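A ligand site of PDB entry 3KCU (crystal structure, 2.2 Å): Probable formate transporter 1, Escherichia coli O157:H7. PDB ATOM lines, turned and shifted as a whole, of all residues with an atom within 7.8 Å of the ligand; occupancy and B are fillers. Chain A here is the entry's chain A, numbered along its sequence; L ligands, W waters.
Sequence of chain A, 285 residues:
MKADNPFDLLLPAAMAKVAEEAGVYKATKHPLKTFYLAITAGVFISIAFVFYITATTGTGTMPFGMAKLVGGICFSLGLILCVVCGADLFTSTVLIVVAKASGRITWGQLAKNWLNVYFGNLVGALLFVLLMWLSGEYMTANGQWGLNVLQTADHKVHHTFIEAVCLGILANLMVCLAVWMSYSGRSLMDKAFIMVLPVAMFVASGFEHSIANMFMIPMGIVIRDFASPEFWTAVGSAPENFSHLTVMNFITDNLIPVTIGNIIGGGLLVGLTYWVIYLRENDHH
An oxygen (O3) of the ligand lies within hydrogen-bond range of the backbone carbonyl oxygen (O) of Lys 112 (2.5 Å).
O of Ala 111 is in hydrogen-bond range of O2 of the ligand (2.8 Å).
The backbone NH of Leu 115 is in hydrogen-bond range of an oxygen (O2) of the ligand, 3.0 Å away.
An oxygen (O2) of the ligand sits at hydrogen-bond distance from the backbone NH (N) of Trp 114.
The indole nitrogen (NE1) of Trp 114 lies within hydrogen-bond range of the backbone carbonyl oxygen (O) of Leu 110.
OH of Tyr 118 sits at hydrogen-bond distance from OG1 of Thr 259, 2.7 Å away.
Merely in contact with the ligand: Tyr 118 (3.6 Å), Phe 90 (3.7 Å) and Asn 113 (3.8 Å).
Hydrophobic or aromatic side chains within 4 Å of the ligand: Phe 90, Trp 114, Leu 115 and Tyr 118.
The nearest printed residue that does not touch the ligand is Thr 259 (4.3 Å).
Water W1 lies within hydrogen-bond range of O2 of the ligand (2.7 Å), N of Asn 116 (3.1 Å), O of Lys 112 (3.1 Å) and N of Leu 115 (3.4 Å).
Water W3 bridges the backbone carbonyl oxygen of Gly 108 (2.7 Å) and an oxygen (O6) of the ligand (2.9 Å).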
ATOM      1  N   PHE A  90     -29.609   0.845 -24.474  1.00  0.00           N
ATOM      2  CA  PHE A  90     -28.359   1.598 -24.666  1.00  0.00           C
ATOM      3  C   PHE A  90     -28.096   2.104 -26.085  1.00  0.00           C
ATOM      4  O   PHE A  90     -27.758   1.321 -26.990  1.00  0.00           O
ATOM      5  CB  PHE A  90     -27.185   0.734 -24.168  1.00  0.00           C
ATOM      6  CG  PHE A  90     -25.838   1.392 -24.289  1.00  0.00           C
ATOM      7  CD1 PHE A  90     -25.541   2.539 -23.564  1.00  0.00           C
ATOM      8  CD2 PHE A  90     -24.861   0.851 -25.115  1.00  0.00           C
ATOM      9  CE1 PHE A  90     -24.288   3.144 -23.661  1.00  0.00           C
ATOM     10  CE2 PHE A  90     -23.593   1.444 -25.225  1.00  0.00           C
ATOM     11  CZ  PHE A  90     -23.317   2.590 -24.496  1.00  0.00           C
ATOM     12  N   THR A  91     -28.225   3.421 -26.253  1.00  0.00           N
ATOM     13  CA  THR A  91     -27.965   4.174 -27.499  1.00  0.00           C
ATOM     14  C   THR A  91     -28.971   3.941 -28.651  1.00  0.00           C
ATOM     15  O   THR A  91     -28.881   4.601 -29.687  1.00  0.00           O
ATOM     16  CB  THR A  91     -26.524   3.960 -28.038  1.00  0.00           C
ATOM     17  OG1 THR A  91     -26.425   2.678 -28.677  1.00  0.00           O
ATOM     18  CG2 THR A  91     -25.484   4.079 -26.918  1.00  0.00           C
ATOM     19  N   TRP A 107     -23.049  16.457 -27.787  1.00  0.00           N
ATOM     20  CA  TRP A 107     -22.748  15.067 -27.419  1.00  0.00           C
ATOM     21  C   TRP A 107     -22.948  14.810 -25.920  1.00  0.00           C
ATOM     22  O   TRP A 107     -23.490  13.776 -25.540  1.00  0.00           O
ATOM     23  CB  TRP A 107     -21.336  14.679 -27.869  1.00  0.00           C
ATOM     24  CG  TRP A 107     -21.292  13.973 -29.216  1.00  0.00           C
ATOM     25  CD1 TRP A 107     -21.724  12.697 -29.486  1.00  0.00           C
ATOM     26  CD2 TRP A 107     -20.793  14.498 -30.453  1.00  0.00           C
ATOM     27  NE1 TRP A 107     -21.525  12.409 -30.823  1.00  0.00           N
ATOM     28  CE2 TRP A 107     -20.944  13.495 -31.432  1.00  0.00           C
ATOM     29  CE3 TRP A 107     -20.227  15.724 -30.819  1.00  0.00           C
ATOM     30  CZ2 TRP A 107     -20.560  13.676 -32.753  1.00  0.00           C
ATOM     31  CZ3 TRP A 107     -19.843  15.906 -32.141  1.00  0.00           C
ATOM     32  CH2 TRP A 107     -20.008  14.892 -33.097  1.00  0.00           C
ATOM     33  N   GLY A 108     -22.516  15.740 -25.085  1.00  0.00           N
ATOM     34  CA  GLY A 108     -22.745  15.624 -23.646  1.00  0.00           C
ATOM     35  C   GLY A 108     -24.216  15.355 -23.345  1.00  0.00           C
ATOM     36  O   GLY A 108     -24.543  14.490 -22.549  1.00  0.00           O
ATOM     37  N   GLN A 109     -25.098  16.097 -24.012  1.00  0.00           N
ATOM     38  CA  GLN A 109     -26.540  15.876 -23.876  1.00  0.00           C
ATOM     39  C   GLN A 109     -26.966  14.497 -24.384  1.00  0.00           C
ATOM     40  O   GLN A 109     -27.734  13.796 -23.717  1.00  0.00           O
ATOM     41  CB  GLN A 109     -27.330  16.988 -24.575  1.00  0.00           C
ATOM     42  CG  GLN A 109     -27.285  18.317 -23.818  1.00  0.00           C
ATOM     43  CD  GLN A 109     -27.904  19.472 -24.596  1.00  0.00           C
ATOM     44  OE1 GLN A 109     -27.670  19.605 -25.801  1.00  0.00           O
ATOM     45  NE2 GLN A 109     -28.670  20.346 -23.917  1.00  0.00           N
ATOM     46  N   LEU A 110     -26.496  14.114 -25.561  1.00  0.00           N
ATOM     47  CA  LEU A 110     -26.797  12.794 -26.099  1.00  0.00           C
ATOM     48  C   LEU A 110     -26.370  11.655 -25.164  1.00  0.00           C
ATOM     49  O   LEU A 110     -27.090  10.672 -25.014  1.00  0.00           O
ATOM     50  CB  LEU A 110     -26.114  12.579 -27.459  1.00  0.00           C
ATOM     51  CG  LEU A 110     -26.705  13.350 -28.655  1.00  0.00           C
ATOM     52  CD1 LEU A 110     -25.863  13.125 -29.911  1.00  0.00           C
ATOM     53  CD2 LEU A 110     -28.174  12.969 -28.876  1.00  0.00           C
ATOM     54  N   ALA A 111     -25.201  11.793 -24.543  1.00  0.00           N
ATOM     55  CA  ALA A 111     -24.616  10.708 -23.735  1.00  0.00           C
ATOM     56  C   ALA A 111     -24.982  10.819 -22.242  1.00  0.00           C
ATOM     57  O   ALA A 111     -24.542  10.008 -21.418  1.00  0.00           O
ATOM     58  CB  ALA A 111     -23.123  10.668 -23.931  1.00  0.00           C
ATOM     59  N   LYS A 112     -25.814  11.797 -21.923  1.00  0.00           N
ATOM     60  CA  LYS A 112     -26.185  12.138 -20.552  1.00  0.00           C
ATOM     61  C   LYS A 112     -26.655  10.955 -19.713  1.00  0.00           C
ATOM     62  O   LYS A 112     -26.348  10.855 -18.532  1.00  0.00           O
ATOM     63  CB  LYS A 112     -27.255  13.243 -20.582  1.00  0.00           C
ATOM     64  CG  LYS A 112     -28.057  13.404 -19.284  1.00  0.00           C
ATOM     65  CD  LYS A 112     -28.389  14.863 -19.014  1.00  0.00           C
ATOM     66  CE  LYS A 112     -28.932  15.574 -20.260  1.00  0.00           C
ATOM     67  NZ  LYS A 112     -29.066  17.039 -20.025  1.00  0.00           N
ATOM     68  N   ASN A 113     -27.423  10.058 -20.314  1.00  0.00           N
ATOM     69  CA  ASN A 113     -27.983   8.953 -19.558  1.00  0.00           C
ATOM     70  C   ASN A 113     -27.336   7.596 -19.880  1.00  0.00           C
ATOM     71  O   ASN A 113     -27.792   6.559 -19.403  1.00  0.00           O
ATOM     72  CB  ASN A 113     -29.499   8.898 -19.768  1.00  0.00           C
ATOM     73  CG  ASN A 113     -30.233   9.964 -18.954  1.00  0.00           C
ATOM     74  OD1 ASN A 113     -31.243  10.496 -19.393  1.00  0.00           O
ATOM     75  ND2 ASN A 113     -29.719  10.266 -17.773  1.00  0.00           N
ATOM     76  N   TRP A 114     -26.278   7.615 -20.677  1.00  0.00           N
ATOM     77  CA  TRP A 114     -25.684   6.368 -21.179  1.00  0.00           C
ATOM     78  C   TRP A 114     -25.190   5.455 -20.063  1.00  0.00           C
ATOM     79  O   TRP A 114     -25.486   4.259 -20.069  1.00  0.00           O
ATOM     80  CB  TRP A 114     -24.567   6.669 -22.168  1.00  0.00           C
ATOM     81  CG  TRP A 114     -25.077   7.072 -23.525  1.00  0.00           C
ATOM     82  CD1 TRP A 114     -26.379   7.252 -23.896  1.00  0.00           C
ATOM     83  CD2 TRP A 114     -24.295   7.326 -24.691  1.00  0.00           C
ATOM     84  NE1 TRP A 114     -26.460   7.613 -25.229  1.00  0.00           N
ATOM     85  CE2 TRP A 114     -25.178   7.664 -25.730  1.00  0.00           C
ATOM     86  CE3 TRP A 114     -22.920   7.314 -24.956  1.00  0.00           C
ATOM     87  CZ2 TRP A 114     -24.737   7.983 -27.015  1.00  0.00           C
ATOM     88  CZ3 TRP A 114     -22.485   7.629 -26.230  1.00  0.00           C
ATOM     89  CH2 TRP A 114     -23.391   7.951 -27.246  1.00  0.00           C
ATOM     90  N   LEU A 115     -24.465   6.008 -19.092  1.00  0.00           N
ATOM     91  CA  LEU A 115     -23.919   5.206 -18.002  1.00  0.00           C
ATOM     92  C   LEU A 115     -25.027   4.484 -17.234  1.00  0.00           C
ATOM     93  O   LEU A 115     -24.969   3.271 -17.009  1.00  0.00           O
ATOM     94  CB  LEU A 115     -23.090   6.052 -17.038  1.00  0.00           C
ATOM     95  CG  LEU A 115     -22.563   5.279 -15.821  1.00  0.00           C
ATOM     96  CD1 LEU A 115     -21.724   4.083 -16.262  1.00  0.00           C
ATOM     97  CD2 LEU A 115     -21.767   6.166 -14.860  1.00  0.00           C
ATOM     98  N   ASN A 116     -26.018   5.267 -16.833  1.00  0.00           N
ATOM     99  CA  ASN A 116     -27.220   4.803 -16.150  1.00  0.00           C
ATOM    100  C   ASN A 116     -27.994   3.720 -16.910  1.00  0.00           C
ATOM    101  O   ASN A 116     -28.368   2.711 -16.325  1.00  0.00           O
ATOM    102  CB  ASN A 116     -28.135   6.019 -15.898  1.00  0.00           C
ATOM    103  CG  ASN A 116     -29.359   5.682 -15.064  1.00  0.00           C
ATOM    104  OD1 ASN A 116     -29.488   4.583 -14.546  1.00  0.00           O
ATOM    105  ND2 ASN A 116     -30.261   6.657 -14.905  1.00  0.00           N
ATOM    106  N   VAL A 117     -28.228   3.951 -18.201  1.00  0.00           N
ATOM    107  CA  VAL A 117     -28.936   2.958 -19.040  1.00  0.00           C
ATOM    108  C   VAL A 117     -28.122   1.670 -19.227  1.00  0.00           C
ATOM    109  O   VAL A 117     -28.643   0.551 -19.159  1.00  0.00           O
ATOM    110  CB  VAL A 117     -29.279   3.554 -20.429  1.00  0.00           C
ATOM    111  CG1 VAL A 117     -29.737   2.460 -21.408  1.00  0.00           C
ATOM    112  CG2 VAL A 117     -30.323   4.719 -20.298  1.00  0.00           C
ATOM    113  N   TYR A 118     -26.831   1.839 -19.480  1.00  0.00           N
ATOM    114  CA  TYR A 118     -25.941   0.720 -19.704  1.00  0.00           C
ATOM    115  C   TYR A 118     -25.963  -0.203 -18.476  1.00  0.00           C
ATOM    116  O   TYR A 118     -26.050  -1.421 -18.612  1.00  0.00           O
ATOM    117  CB  TYR A 118     -24.536   1.262 -19.922  1.00  0.00           C
ATOM    118  CG  TYR A 118     -23.491   0.276 -20.381  1.00  0.00           C
ATOM    119  CD1 TYR A 118     -23.333  -0.029 -21.743  1.00  0.00           C
ATOM    120  CD2 TYR A 118     -22.596  -0.311 -19.466  1.00  0.00           C
ATOM    121  CE1 TYR A 118     -22.339  -0.895 -22.188  1.00  0.00           C
ATOM    122  CE2 TYR A 118     -21.607  -1.183 -19.890  1.00  0.00           C
ATOM    123  CZ  TYR A 118     -21.481  -1.470 -21.246  1.00  0.00           C
ATOM    124  OH  TYR A 118     -20.503  -2.347 -21.679  1.00  0.00           O
ATOM    125  N   PHE A 119     -25.917   0.414 -17.301  1.00  0.00           N
ATOM    126  CA  PHE A 119     -25.936  -0.287 -16.025  1.00  0.00           C
ATOM    127  C   PHE A 119     -27.262  -1.001 -15.818  1.00  0.00           C
ATOM    128  O   PHE A 119     -27.300  -2.206 -15.524  1.00  0.00           O
ATOM    129  CB  PHE A 119     -25.677   0.693 -14.873  1.00  0.00           C
ATOM    130  CG  PHE A 119     -25.659   0.056 -13.509  1.00  0.00           C
ATOM    131  CD1 PHE A 119     -24.754  -0.943 -13.212  1.00  0.00           C
ATOM    132  CD2 PHE A 119     -26.524   0.498 -12.524  1.00  0.00           C
ATOM    133  CE1 PHE A 119     -24.727  -1.517 -11.939  1.00  0.00           C
ATOM    134  CE2 PHE A 119     -26.497  -0.076 -11.251  1.00  0.00           C
ATOM    135  CZ  PHE A 119     -25.606  -1.070 -10.961  1.00  0.00           C
ATOM    136  N   SER A 210     -23.538  -5.144 -27.422  1.00  0.00           N
ATOM    137  CA  SER A 210     -23.056  -5.227 -26.017  1.00  0.00           C
ATOM    138  C   SER A 210     -24.097  -5.677 -24.985  1.00  0.00           C
ATOM    139  O   SER A 210     -23.803  -6.502 -24.115  1.00  0.00           O
ATOM    140  CB  SER A 210     -22.463  -3.879 -25.570  1.00  0.00           C
ATOM    141  OG  SER A 210     -23.397  -2.826 -25.788  1.00  0.00           O
ATOM    142  N   ILE A 211     -25.307  -5.144 -25.094  1.00  0.00           N
ATOM    143  CA  ILE A 211     -26.377  -5.483 -24.155  1.00  0.00           C
ATOM    144  C   ILE A 211     -26.869  -6.911 -24.379  1.00  0.00           C
ATOM    145  O   ILE A 211     -27.029  -7.677 -23.416  1.00  0.00           O
ATOM    146  CB  ILE A 211     -27.548  -4.503 -24.233  1.00  0.00           C
ATOM    147  CG1 ILE A 211     -27.022  -3.052 -24.227  1.00  0.00           C
ATOM    148  CG2 ILE A 211     -28.533  -4.747 -23.082  1.00  0.00           C
ATOM    149  CD1 ILE A 211     -26.176  -2.732 -22.993  1.00  0.00           C
ATOM    150  N   MET A 214     -24.619  -9.153 -22.705  1.00  0.00           N
ATOM    151  CA  MET A 214     -24.722  -9.138 -21.253  1.00  0.00           C
ATOM    152  C   MET A 214     -25.627 -10.267 -20.812  1.00  0.00           C
ATOM    153  O   MET A 214     -25.519 -10.757 -19.682  1.00  0.00           O
ATOM    154  CB  MET A 214     -25.303  -7.813 -20.771  1.00  0.00           C
ATOM    155  CG  MET A 214     -24.352  -6.672 -20.874  1.00  0.00           C
ATOM    156  SD  MET A 214     -25.161  -5.144 -20.414  1.00  0.00           S
ATOM    157  CE  MET A 214     -23.783  -4.007 -20.440  1.00  0.00           C
ATOM    158  N   THR A 259     -18.514  -2.669 -26.874  1.00  0.00           N
ATOM    159  CA  THR A 259     -19.184  -1.472 -26.371  1.00  0.00           C
ATOM    160  C   THR A 259     -18.612  -0.260 -27.115  1.00  0.00           C
ATOM    161  O   THR A 259     -19.351   0.589 -27.600  1.00  0.00           O
ATOM    162  CB  THR A 259     -19.071  -1.344 -24.841  1.00  0.00           C
ATOM    163  OG1 THR A 259     -19.640  -2.515 -24.228  1.00  0.00           O
ATOM    164  CG2 THR A 259     -19.791  -0.073 -24.326  1.00  0.00           C
ATOM    165  N   ILE A 260     -17.293  -0.238 -27.257  1.00  0.00           N
ATOM    166  CA  ILE A 260     -16.638   0.785 -28.054  1.00  0.00           C
ATOM    167  C   ILE A 260     -17.172   0.869 -29.491  1.00  0.00           C
ATOM    168  O   ILE A 260     -17.543   1.952 -29.961  1.00  0.00           O
ATOM    169  CB  ILE A 260     -15.116   0.584 -28.028  1.00  0.00           C
ATOM    170  CG1 ILE A 260     -14.588   0.886 -26.616  1.00  0.00           C
ATOM    171  CG2 ILE A 260     -14.445   1.458 -29.088  1.00  0.00           C
ATOM    172  CD1 ILE A 260     -13.138   0.533 -26.410  1.00  0.00           C
ATOM    173  N   ILE A 263     -20.766   2.243 -29.701  1.00  0.00           N
ATOM    174  CA  ILE A 263     -20.784   3.700 -29.558  1.00  0.00           C
ATOM    175  C   ILE A 263     -20.312   4.388 -30.844  1.00  0.00           C
ATOM    176  O   ILE A 263     -20.878   5.399 -31.272  1.00  0.00           O
ATOM    177  CB  ILE A 263     -19.889   4.160 -28.408  1.00  0.00           C
ATOM    178  CG1 ILE A 263     -20.437   3.652 -27.060  1.00  0.00           C
ATOM    179  CG2 ILE A 263     -19.731   5.694 -28.414  1.00  0.00           C
ATOM    180  CD1 ILE A 263     -19.463   3.910 -25.881  1.00  0.00           C
HETATM  181  C1  LIG L   1     -21.363   4.508 -21.738  1.00  0.00           C
HETATM  182  C2  LIG L   1     -21.345   3.036 -21.343  1.00  0.00           C
HETATM  183  C3  LIG L   1     -19.941   2.625 -20.968  1.00  0.00           C
HETATM  184  C4  LIG L   1     -19.540   3.430 -19.737  1.00  0.00           C
HETATM  185  C5  LIG L   1     -19.512   4.926 -20.047  1.00  0.00           C
HETATM  186  C6  LIG L   1     -20.793   5.458 -20.683  1.00  0.00           C
HETATM  187  C7  LIG L   1     -20.434   6.758 -21.385  1.00  0.00           C
HETATM  188  C8  LIG L   1     -20.159   7.879 -20.383  1.00  0.00           C
HETATM  189  O1  LIG L   1     -21.287   8.052 -19.514  1.00  0.00           O
HETATM  190  C9  LIG L   1     -21.638   9.434 -19.417  1.00  0.00           C
HETATM  191  C10 LIG L   1     -22.774   9.619 -18.414  1.00  0.00           C
HETATM  192  O2  LIG L   1     -23.946   8.922 -18.854  1.00  0.00           O
HETATM  193  C11 LIG L   1     -23.081  11.107 -18.259  1.00  0.00           C
HETATM  194  O3  LIG L   1     -24.170  11.306 -17.346  1.00  0.00           O
HETATM  195  O4  LIG L   1     -20.484  10.158 -19.003  1.00  0.00           O
HETATM  196  C12 LIG L   1     -20.661  11.555 -18.763  1.00  0.00           C
HETATM  197  C13 LIG L   1     -19.358  12.110 -18.200  1.00  0.00           C
HETATM  198  O5  LIG L   1     -19.155  11.652 -16.862  1.00  0.00           O
HETATM  199  C14 LIG L   1     -21.816  11.827 -17.804  1.00  0.00           C
HETATM  200  O6  LIG L   1     -22.008  13.240 -17.754  1.00  0.00           O
HETATM  201  C15 LIG L   1     -22.661  13.709 -16.572  1.00  0.00           C
HETATM  202  O7  LIG L   1     -21.710  13.699 -15.512  1.00  0.00           O
HETATM  203  C16 LIG L   1     -20.555  14.494 -15.797  1.00  0.00           C
HETATM  204  C17 LIG L   1     -19.577  14.403 -14.622  1.00  0.00           C
HETATM  205  O8  LIG L   1     -18.241  14.392 -15.135  1.00  0.00           O
HETATM  206  C18 LIG L   1     -20.927  15.951 -16.089  1.00  0.00           C
HETATM  207  O9  LIG L   1     -19.758  16.674 -16.461  1.00  0.00           O
HETATM  208  C19 LIG L   1     -21.941  15.994 -17.218  1.00  0.00           C
HETATM  209  O10 LIG L   1     -22.322  17.343 -17.502  1.00  0.00           O
HETATM  210  C20 LIG L   1     -23.136  15.139 -16.806  1.00  0.00           C
HETATM  211  O11 LIG L   1     -24.171  15.176 -17.800  1.00  0.00           O
HETATM  212  O   HOH W   1     -25.731   8.307 -16.914  1.00  0.00           O
HETATM  213  O   HOH W   2     -20.519  19.079 -18.759  1.00  0.00           O
HETATM  214  O   HOH W   3     -23.215  13.610 -20.391  1.00  0.00           O
